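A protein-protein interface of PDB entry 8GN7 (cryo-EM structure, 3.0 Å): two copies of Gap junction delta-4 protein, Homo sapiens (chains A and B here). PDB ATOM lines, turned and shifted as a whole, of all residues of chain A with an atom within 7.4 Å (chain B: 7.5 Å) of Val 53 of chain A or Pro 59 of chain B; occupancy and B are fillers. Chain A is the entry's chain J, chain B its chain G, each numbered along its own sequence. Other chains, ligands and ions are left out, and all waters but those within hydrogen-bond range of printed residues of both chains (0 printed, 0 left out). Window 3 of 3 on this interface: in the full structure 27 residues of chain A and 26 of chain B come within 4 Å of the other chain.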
ATOM      1  N   GLU A  48     -28.814 -32.749  -4.875  1.00  0.00           N
ATOM      2  CA  GLU A  48     -29.351 -32.092  -3.688  1.00  0.00           C
ATOM      3  C   GLU A  48     -28.682 -32.588  -2.414  1.00  0.00           C
ATOM      4  O   GLU A  48     -28.465 -31.802  -1.486  1.00  0.00           O
ATOM      5  CB  GLU A  48     -30.863 -32.300  -3.612  1.00  0.00           C
ATOM      6  CG  GLU A  48     -31.335 -33.633  -4.156  1.00  0.00           C
ATOM      7  CD  GLU A  48     -32.713 -34.010  -3.652  1.00  0.00           C
ATOM      8  OE1 GLU A  48     -33.284 -33.240  -2.852  1.00  0.00           O
ATOM      9  OE2 GLU A  48     -33.222 -35.077  -4.050  1.00  0.00           O
ATOM     10  N   GLN A  49     -28.353 -33.878  -2.343  1.00  0.00           N
ATOM     11  CA  GLN A  49     -27.651 -34.432  -1.190  1.00  0.00           C
ATOM     12  C   GLN A  49     -26.143 -34.478  -1.375  1.00  0.00           C
ATOM     13  O   GLN A  49     -25.406 -34.348  -0.393  1.00  0.00           O
ATOM     14  CB  GLN A  49     -28.158 -35.844  -0.882  1.00  0.00           C
ATOM     15  CG  GLN A  49     -27.584 -36.442   0.395  1.00  0.00           C
ATOM     16  CD  GLN A  49     -28.045 -37.863   0.641  1.00  0.00           C
ATOM     17  OE1 GLN A  49     -28.454 -38.564  -0.282  1.00  0.00           O
ATOM     18  NE2 GLN A  49     -27.979 -38.295   1.893  1.00  0.00           N
ATOM     19  N   GLU A  50     -25.672 -34.653  -2.610  1.00  0.00           N
ATOM     20  CA  GLU A  50     -24.235 -34.720  -2.855  1.00  0.00           C
ATOM     21  C   GLU A  50     -23.549 -33.408  -2.494  1.00  0.00           C
ATOM     22  O   GLU A  50     -22.451 -33.411  -1.926  1.00  0.00           O
ATOM     23  CB  GLU A  50     -23.972 -35.081  -4.316  1.00  0.00           C
ATOM     24  CG  GLU A  50     -22.506 -35.276  -4.654  1.00  0.00           C
ATOM     25  CD  GLU A  50     -22.135 -34.686  -6.000  1.00  0.00           C
ATOM     26  OE1 GLU A  50     -22.959 -34.772  -6.935  1.00  0.00           O
ATOM     27  OE2 GLU A  50     -21.021 -34.136  -6.122  1.00  0.00           O
ATOM     28  N   ARG A  51     -24.176 -32.279  -2.812  1.00  0.00           N
ATOM     29  CA  ARG A  51     -23.623 -30.962  -2.529  1.00  0.00           C
ATOM     30  C   ARG A  51     -24.413 -30.254  -1.435  1.00  0.00           C
ATOM     31  O   ARG A  51     -24.637 -29.045  -1.486  1.00  0.00           O
ATOM     32  CB  ARG A  51     -23.567 -30.109  -3.793  1.00  0.00           C
ATOM     33  CG  ARG A  51     -22.679 -30.686  -4.881  1.00  0.00           C
ATOM     34  CD  ARG A  51     -21.211 -30.409  -4.603  1.00  0.00           C
ATOM     35  NE  ARG A  51     -20.770 -29.137  -5.162  1.00  0.00           N
ATOM     36  CZ  ARG A  51     -20.104 -28.213  -4.485  1.00  0.00           C
ATOM     37  NH1 ARG A  51     -19.785 -28.383  -3.213  1.00  0.00           N
ATOM     38  NH2 ARG A  51     -19.749 -27.087  -5.099  1.00  0.00           N
ATOM     39  N   PHE A  52     -24.849 -31.011  -0.430  1.00  0.00           N
ATOM     40  CA  PHE A  52     -25.449 -30.458   0.783  1.00  0.00           C
ATOM     41  C   PHE A  52     -24.353 -30.486   1.843  1.00  0.00           C
ATOM     42  O   PHE A  52     -24.223 -31.443   2.606  1.00  0.00           O
ATOM     43  CB  PHE A  52     -26.681 -31.255   1.196  1.00  0.00           C
ATOM     44  CG  PHE A  52     -27.385 -30.715   2.409  1.00  0.00           C
ATOM     45  CD1 PHE A  52     -28.270 -29.658   2.298  1.00  0.00           C
ATOM     46  CD2 PHE A  52     -27.178 -31.279   3.656  1.00  0.00           C
ATOM     47  CE1 PHE A  52     -28.924 -29.165   3.408  1.00  0.00           C
ATOM     48  CE2 PHE A  52     -27.832 -30.787   4.768  1.00  0.00           C
ATOM     49  CZ  PHE A  52     -28.706 -29.730   4.643  1.00  0.00           C
ATOM     50  N   VAL A  53     -23.553 -29.425   1.879  1.00  0.00           N
ATOM     51  CA  VAL A  53     -22.311 -29.406   2.643  1.00  0.00           C
ATOM     52  C   VAL A  53     -22.595 -28.929   4.060  1.00  0.00           C
ATOM     53  O   VAL A  53     -23.147 -27.843   4.261  1.00  0.00           O
ATOM     54  CB  VAL A  53     -21.261 -28.515   1.963  1.00  0.00           C
ATOM     55  CG1 VAL A  53     -20.113 -28.230   2.913  1.00  0.00           C
ATOM     56  CG2 VAL A  53     -20.755 -29.171   0.690  1.00  0.00           C
ATOM     57  N   CYS A  54     -22.211 -29.740   5.041  1.00  0.00           N
ATOM     58  CA  CYS A  54     -22.302 -29.392   6.450  1.00  0.00           C
ATOM     59  C   CYS A  54     -20.906 -29.174   7.024  1.00  0.00           C
ATOM     60  O   CYS A  54     -19.904 -29.646   6.484  1.00  0.00           O
ATOM     61  CB  CYS A  54     -23.031 -30.486   7.235  1.00  0.00           C
ATOM     62  SG  CYS A  54     -24.774 -30.697   6.795  1.00  0.00           S
ATOM     63  N   ASN A  55     -20.852 -28.442   8.136  1.00  0.00           N
ATOM     64  CA  ASN A  55     -19.586 -28.074   8.770  1.00  0.00           C
ATOM     65  C   ASN A  55     -19.281 -29.083   9.874  1.00  0.00           C
ATOM     66  O   ASN A  55     -19.397 -28.802  11.067  1.00  0.00           O
ATOM     67  CB  ASN A  55     -19.658 -26.647   9.305  1.00  0.00           C
ATOM     68  CG  ASN A  55     -18.299 -26.091   9.682  1.00  0.00           C
ATOM     69  OD1 ASN A  55     -17.414 -26.819  10.128  1.00  0.00           O
ATOM     70  ND2 ASN A  55     -18.127 -24.787   9.504  1.00  0.00           N
ATOM     71  N   THR A  56     -18.871 -30.280   9.459  1.00  0.00           N
ATOM     72  CA  THR A  56     -18.549 -31.343  10.401  1.00  0.00           C
ATOM     73  C   THR A  56     -17.610 -32.335   9.732  1.00  0.00           C
ATOM     74  O   THR A  56     -17.473 -32.360   8.506  1.00  0.00           O
ATOM     75  CB  THR A  56     -19.810 -32.053  10.904  1.00  0.00           C
ATOM     76  OG1 THR A  56     -19.500 -32.815  12.078  1.00  0.00           O
ATOM     77  CG2 THR A  56     -20.364 -32.981   9.835  1.00  0.00           C
ATOM     78  N   ALA A  62     -23.780 -35.823   8.315  1.00  0.00           N
ATOM     79  CA  ALA A  62     -24.351 -35.275   7.094  1.00  0.00           C
ATOM     80  C   ALA A  62     -25.575 -36.039   6.613  1.00  0.00           C
ATOM     81  O   ALA A  62     -26.491 -35.422   6.059  1.00  0.00           O
ATOM     82  CB  ALA A  62     -23.299 -35.250   5.983  1.00  0.00           C
ATOM     83  N   PHE A 173     -29.277 -24.143   6.887  1.00  0.00           N
ATOM     84  CA  PHE A 173     -30.011 -25.013   7.797  1.00  0.00           C
ATOM     85  C   PHE A 173     -29.218 -25.275   9.073  1.00  0.00           C
ATOM     86  O   PHE A 173     -28.064 -25.722   9.009  1.00  0.00           O
ATOM     87  CB  PHE A 173     -30.352 -26.336   7.111  1.00  0.00           C
ATOM     88  CG  PHE A 173     -31.234 -27.236   7.928  1.00  0.00           C
ATOM     89  CD1 PHE A 173     -32.532 -26.864   8.231  1.00  0.00           C
ATOM     90  CD2 PHE A 173     -30.763 -28.449   8.399  1.00  0.00           C
ATOM     91  CE1 PHE A 173     -33.343 -27.687   8.985  1.00  0.00           C
ATOM     92  CE2 PHE A 173     -31.570 -29.273   9.154  1.00  0.00           C
ATOM     93  CZ  PHE A 173     -32.861 -28.892   9.447  1.00  0.00           C
ATOM     94  N   VAL A 184     -24.599 -27.409  14.120  1.00  0.00           N
ATOM     95  CA  VAL A 184     -23.910 -27.449  12.836  1.00  0.00           C
ATOM     96  C   VAL A 184     -24.710 -26.643  11.825  1.00  0.00           C
ATOM     97  O   VAL A 184     -25.942 -26.585  11.878  1.00  0.00           O
ATOM     98  CB  VAL A 184     -23.707 -28.903  12.361  1.00  0.00           C
ATOM     99  CG1 VAL A 184     -22.680 -28.965  11.247  1.00  0.00           C
ATOM    100  CG2 VAL A 184     -23.284 -29.783  13.524  1.00  0.00           C
ATOM    101  N   ASP A 185     -24.004 -26.003  10.898  1.00  0.00           N
ATOM    102  CA  ASP A 185     -24.622 -25.229   9.832  1.00  0.00           C
ATOM    103  C   ASP A 185     -24.400 -25.936   8.505  1.00  0.00           C
ATOM    104  O   ASP A 185     -23.277 -26.356   8.204  1.00  0.00           O
ATOM    105  CB  ASP A 185     -24.052 -23.810   9.779  1.00  0.00           C
ATOM    106  CG  ASP A 185     -24.632 -22.908  10.850  1.00  0.00           C
ATOM    107  OD1 ASP A 185     -25.758 -22.404  10.659  1.00  0.00           O
ATOM    108  OD2 ASP A 185     -23.959 -22.701  11.881  1.00  0.00           O
ATOM    109  N   CYS A 186     -25.463 -26.069   7.715  1.00  0.00           N
ATOM    110  CA  CYS A 186     -25.386 -26.705   6.411  1.00  0.00           C
ATOM    111  C   CYS A 186     -25.926 -25.762   5.347  1.00  0.00           C
ATOM    112  O   CYS A 186     -26.786 -24.921   5.618  1.00  0.00           O
ATOM    113  CB  CYS A 186     -26.154 -28.030   6.384  1.00  0.00           C
ATOM    114  SG  CYS A 186     -25.734 -29.166   7.726  1.00  0.00           S
ATOM    115  N   TYR A 187     -25.410 -25.914   4.131  1.00  0.00           N
ATOM    116  CA  TYR A 187     -25.704 -25.017   3.022  1.00  0.00           C
ATOM    117  C   TYR A 187     -26.505 -25.756   1.960  1.00  0.00           C
ATOM    118  O   TYR A 187     -26.181 -26.896   1.612  1.00  0.00           O
ATOM    119  CB  TYR A 187     -24.413 -24.460   2.420  1.00  0.00           C
ATOM    120  CG  TYR A 187     -23.713 -23.457   3.309  1.00  0.00           C
ATOM    121  CD1 TYR A 187     -22.825 -23.873   4.292  1.00  0.00           C
ATOM    122  CD2 TYR A 187     -23.940 -22.096   3.166  1.00  0.00           C
ATOM    123  CE1 TYR A 187     -22.187 -22.962   5.107  1.00  0.00           C
ATOM    124  CE2 TYR A 187     -23.304 -21.178   3.976  1.00  0.00           C
ATOM    125  CZ  TYR A 187     -22.429 -21.617   4.945  1.00  0.00           C
ATOM    126  OH  TYR A 187     -21.793 -20.704   5.753  1.00  0.00           O
ATOM    127  N   VAL A 188     -27.543 -25.105   1.448  1.00  0.00           N
ATOM    128  CA  VAL A 188     -28.403 -25.696   0.429  1.00  0.00           C
ATOM    129  C   VAL A 188     -27.810 -25.431  -0.948  1.00  0.00           C
ATOM    130  O   VAL A 188     -27.311 -24.335  -1.228  1.00  0.00           O
ATOM    131  CB  VAL A 188     -29.832 -25.137   0.545  1.00  0.00           C
ATOM    132  CG1 VAL A 188     -30.732 -25.726  -0.530  1.00  0.00           C
ATOM    133  CG2 VAL A 188     -30.397 -25.413   1.927  1.00  0.00           C
ATOM    134  N   SER A 189     -27.860 -26.441  -1.814  1.00  0.00           N
ATOM    135  CA  SER A 189     -27.337 -26.318  -3.168  1.00  0.00           C
ATOM    136  C   SER A 189     -28.371 -25.673  -4.083  1.00  0.00           C
ATOM    137  O   SER A 189     -29.544 -26.058  -4.075  1.00  0.00           O
ATOM    138  CB  SER A 189     -26.939 -27.692  -3.705  1.00  0.00           C
ATOM    139  OG  SER A 189     -26.997 -27.722  -5.118  1.00  0.00           O
ATOM    140  N   THR B  56     -10.239 -22.510  -2.349  1.00  0.00           N
ATOM    141  CA  THR B  56     -10.580 -22.299  -0.948  1.00  0.00           C
ATOM    142  C   THR B  56     -10.750 -23.649  -0.267  1.00  0.00           C
ATOM    143  O   THR B  56     -10.902 -24.682  -0.924  1.00  0.00           O
ATOM    144  CB  THR B  56     -11.853 -21.459  -0.796  1.00  0.00           C
ATOM    145  OG1 THR B  56     -11.937 -20.948   0.539  1.00  0.00           O
ATOM    146  CG2 THR B  56     -13.087 -22.295  -1.093  1.00  0.00           C
ATOM    147  N   LEU B  57     -10.714 -23.624   1.067  1.00  0.00           N
ATOM    148  CA  LEU B  57     -10.936 -24.815   1.873  1.00  0.00           C
ATOM    149  C   LEU B  57     -12.053 -24.655   2.893  1.00  0.00           C
ATOM    150  O   LEU B  57     -12.403 -25.635   3.558  1.00  0.00           O
ATOM    151  CB  LEU B  57      -9.647 -25.224   2.604  1.00  0.00           C
ATOM    152  CG  LEU B  57      -8.443 -25.644   1.758  1.00  0.00           C
ATOM    153  CD1 LEU B  57      -7.187 -25.683   2.607  1.00  0.00           C
ATOM    154  CD2 LEU B  57      -8.689 -26.993   1.109  1.00  0.00           C
ATOM    155  N   GLN B  58     -12.616 -23.464   3.041  1.00  0.00           N
ATOM    156  CA  GLN B  58     -13.681 -23.248   4.012  1.00  0.00           C
ATOM    157  C   GLN B  58     -14.998 -23.788   3.467  1.00  0.00           C
ATOM    158  O   GLN B  58     -15.385 -23.442   2.346  1.00  0.00           O
ATOM    159  CB  GLN B  58     -13.814 -21.764   4.337  1.00  0.00           C
ATOM    160  CG  GLN B  58     -15.170 -21.367   4.890  1.00  0.00           C
ATOM    161  CD  GLN B  58     -15.241 -21.489   6.399  1.00  0.00           C
ATOM    162  OE1 GLN B  58     -14.220 -21.464   7.084  1.00  0.00           O
ATOM    163  NE2 GLN B  58     -16.451 -21.627   6.925  1.00  0.00           N
ATOM    164  N   PRO B  59     -15.696 -24.646   4.210  1.00  0.00           N
ATOM    165  CA  PRO B  59     -16.979 -25.168   3.725  1.00  0.00           C
ATOM    166  C   PRO B  59     -17.988 -24.054   3.491  1.00  0.00           C
ATOM    167  O   PRO B  59     -18.054 -23.079   4.241  1.00  0.00           O
ATOM    168  CB  PRO B  59     -17.435 -26.106   4.848  1.00  0.00           C
ATOM    169  CG  PRO B  59     -16.215 -26.436   5.617  1.00  0.00           C
ATOM    170  CD  PRO B  59     -15.230 -25.327   5.430  1.00  0.00           C
ATOM    171  N   GLY B  60     -18.784 -24.212   2.433  1.00  0.00           N
ATOM    172  CA  GLY B  60     -19.832 -23.273   2.106  1.00  0.00           C
ATOM    173  C   GLY B  60     -19.434 -22.154   1.169  1.00  0.00           C
ATOM    174  O   GLY B  60     -20.316 -21.443   0.674  1.00  0.00           O
ATOM    175  N   CYS B  61     -18.139 -21.969   0.908  1.00  0.00           N
ATOM    176  CA  CYS B  61     -17.711 -20.917  -0.007  1.00  0.00           C
ATOM    177  C   CYS B  61     -17.989 -21.277  -1.462  1.00  0.00           C
ATOM    178  O   CYS B  61     -18.430 -20.418  -2.237  1.00  0.00           O
ATOM    179  CB  CYS B  61     -16.222 -20.626   0.192  1.00  0.00           C
ATOM    180  SG  CYS B  61     -15.511 -19.455  -0.984  1.00  0.00           S
ATOM    181  N   ALA B  62     -17.748 -22.529  -1.847  1.00  0.00           N
ATOM    182  CA  ALA B  62     -17.972 -22.981  -3.212  1.00  0.00           C
ATOM    183  C   ALA B  62     -19.443 -22.994  -3.603  1.00  0.00           C
ATOM    184  O   ALA B  62     -19.754 -22.814  -4.785  1.00  0.00           O
ATOM    185  CB  ALA B  62     -17.382 -24.379  -3.410  1.00  0.00           C
ATOM    186  N   ASN B  63     -20.349 -23.209  -2.651  1.00  0.00           N
ATOM    187  CA  ASN B  63     -21.776 -23.136  -2.931  1.00  0.00           C
ATOM    188  C   ASN B  63     -22.222 -21.708  -3.212  1.00  0.00           C
ATOM    189  O   ASN B  63     -22.921 -21.457  -4.200  1.00  0.00           O
ATOM    190  CB  ASN B  63     -22.572 -23.706  -1.754  1.00  0.00           C
ATOM    191  CG  ASN B  63     -22.806 -25.198  -1.874  1.00  0.00           C
ATOM    192  OD1 ASN B  63     -22.103 -25.891  -2.605  1.00  0.00           O
ATOM    193  ND2 ASN B  63     -23.797 -25.699  -1.150  1.00  0.00           N
ATOM    194  N   VAL B  64     -21.810 -20.766  -2.361  1.00  0.00           N
ATOM    195  CA  VAL B  64     -22.179 -19.367  -2.545  1.00  0.00           C
ATOM    196  C   VAL B  64     -21.577 -18.818  -3.831  1.00  0.00           C
ATOM    197  O   VAL B  64     -22.241 -18.095  -4.583  1.00  0.00           O
ATOM    198  CB  VAL B  64     -21.749 -18.541  -1.320  1.00  0.00           C
ATOM    199  CG1 VAL B  64     -22.088 -17.076  -1.520  1.00  0.00           C
ATOM    200  CG2 VAL B  64     -22.407 -19.075  -0.061  1.00  0.00           C
ATOM    201  N   PRO B 179     -18.870 -16.813   3.106  1.00  0.00           N
ATOM    202  CA  PRO B 179     -17.813 -16.718   4.122  1.00  0.00           C
ATOM    203  C   PRO B 179     -16.400 -16.765   3.550  1.00  0.00           C
ATOM    204  O   PRO B 179     -15.440 -16.935   4.295  1.00  0.00           O
ATOM    205  CB  PRO B 179     -18.097 -17.939   5.003  1.00  0.00           C
ATOM    206  CG  PRO B 179     -18.596 -18.962   4.030  1.00  0.00           C
ATOM    207  CD  PRO B 179     -19.392 -18.188   3.001  1.00  0.00           C
ATOM    208  N   CYS B 180     -16.238 -16.628   2.238  1.00  0.00           N
ATOM    209  CA  CYS B 180     -14.905 -16.608   1.653  1.00  0.00           C
ATOM    210  C   CYS B 180     -14.153 -15.356   2.086  1.00  0.00           C
ATOM    211  O   CYS B 180     -14.711 -14.256   2.121  1.00  0.00           O
ATOM    212  CB  CYS B 180     -14.991 -16.674   0.129  1.00  0.00           C
ATOM    213  SG  CYS B 180     -16.361 -17.676  -0.498  1.00  0.00           S
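The side-chain amide oxygen of Asn 63 of chain B is in hydrogen-bond range of the guanidinium group of Arg 51 of chain A.
SG of Cys 54 of chain A forms a disulfide with SG of Cys 186 of chain A, at 2.0 Å.
The backbone NH of Tyr 187 of chain A lies within hydrogen-bond range of the backbone carbonyl oxygen of Val 53 of chain A (3.0 Å).
SG of Cys 61 of chain B forms a disulfide with SG of Cys 180 of chain B, 2.0 Å away.
Ala 62 of chain B touches Arg 51 of chain A.
CG1 of Val 53 of chain A touches CB of Pro 59 of chain B, at 3.9 Å.
CD1 of Tyr 187 of chain A touches CA of Gly 60 of chain B (3.8 Å).
Asn 63 of chain B touches Tyr 187 of chain A (ND2 to CB, 3.8 Å).
Asn 63 of chain B touches Val 188 of chain A (ND2 to O, 3.8 Å).
Of the printed residues of chain B, Arg 51 of chain A touches Ala 62 (3.97 Å) and Asn 63 (3.5 Å).
Val 53 of chain A touches just one residue of chain B: Pro 59 (3.9 Å).
Printed residues of chain B within 4 Å of Tyr 187 of chain A: Gly 60 and Asn 63.
Ser 189 of chain A touches none of the printed residues of chain B.
Thr 56 of chain B touches none of the printed residues of chain A.
Printed residues of chain A within 4 Å of Pro 59 of chain B: Val 53 (3.9 Å).
The nearest residue of chain B that does not touch Val 53 of chain A is Gly 60 of chain B (4.3 Å).
The nearest residue of chain A that does not touch Pro 59 of chain B is Tyr 187 of chain A (4.2 Å).
The nearest printed residue of chain A that does not touch Gly 60 of chain B is Val 53 of chain A (4.3 Å).
Of the 11 printed residues of chain B, 4 touch a printed residue of chain A.
Printed residues of chain B that touch a printed residue of chain A: Pro 59, Gly 60, Ala 62 and Asn 63.
Hydrophobic or aromatic side chains of chain B within 4 Å of the printed part of chain A: Pro 59 and Ala 62.
Along chain B the printed residues that touch a printed residue of chain A span positions 59 to 63.
Among the printed residues, no Asp or Glu carboxylate lies within 4 Å of a Lys or Arg side-chain nitrogen of the other chain.
Positions printed for both chains: 56 and 62.
Of the 6 pairs that touch across the chains among the printed residues, none has its exchanged pair printed and touching as well.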
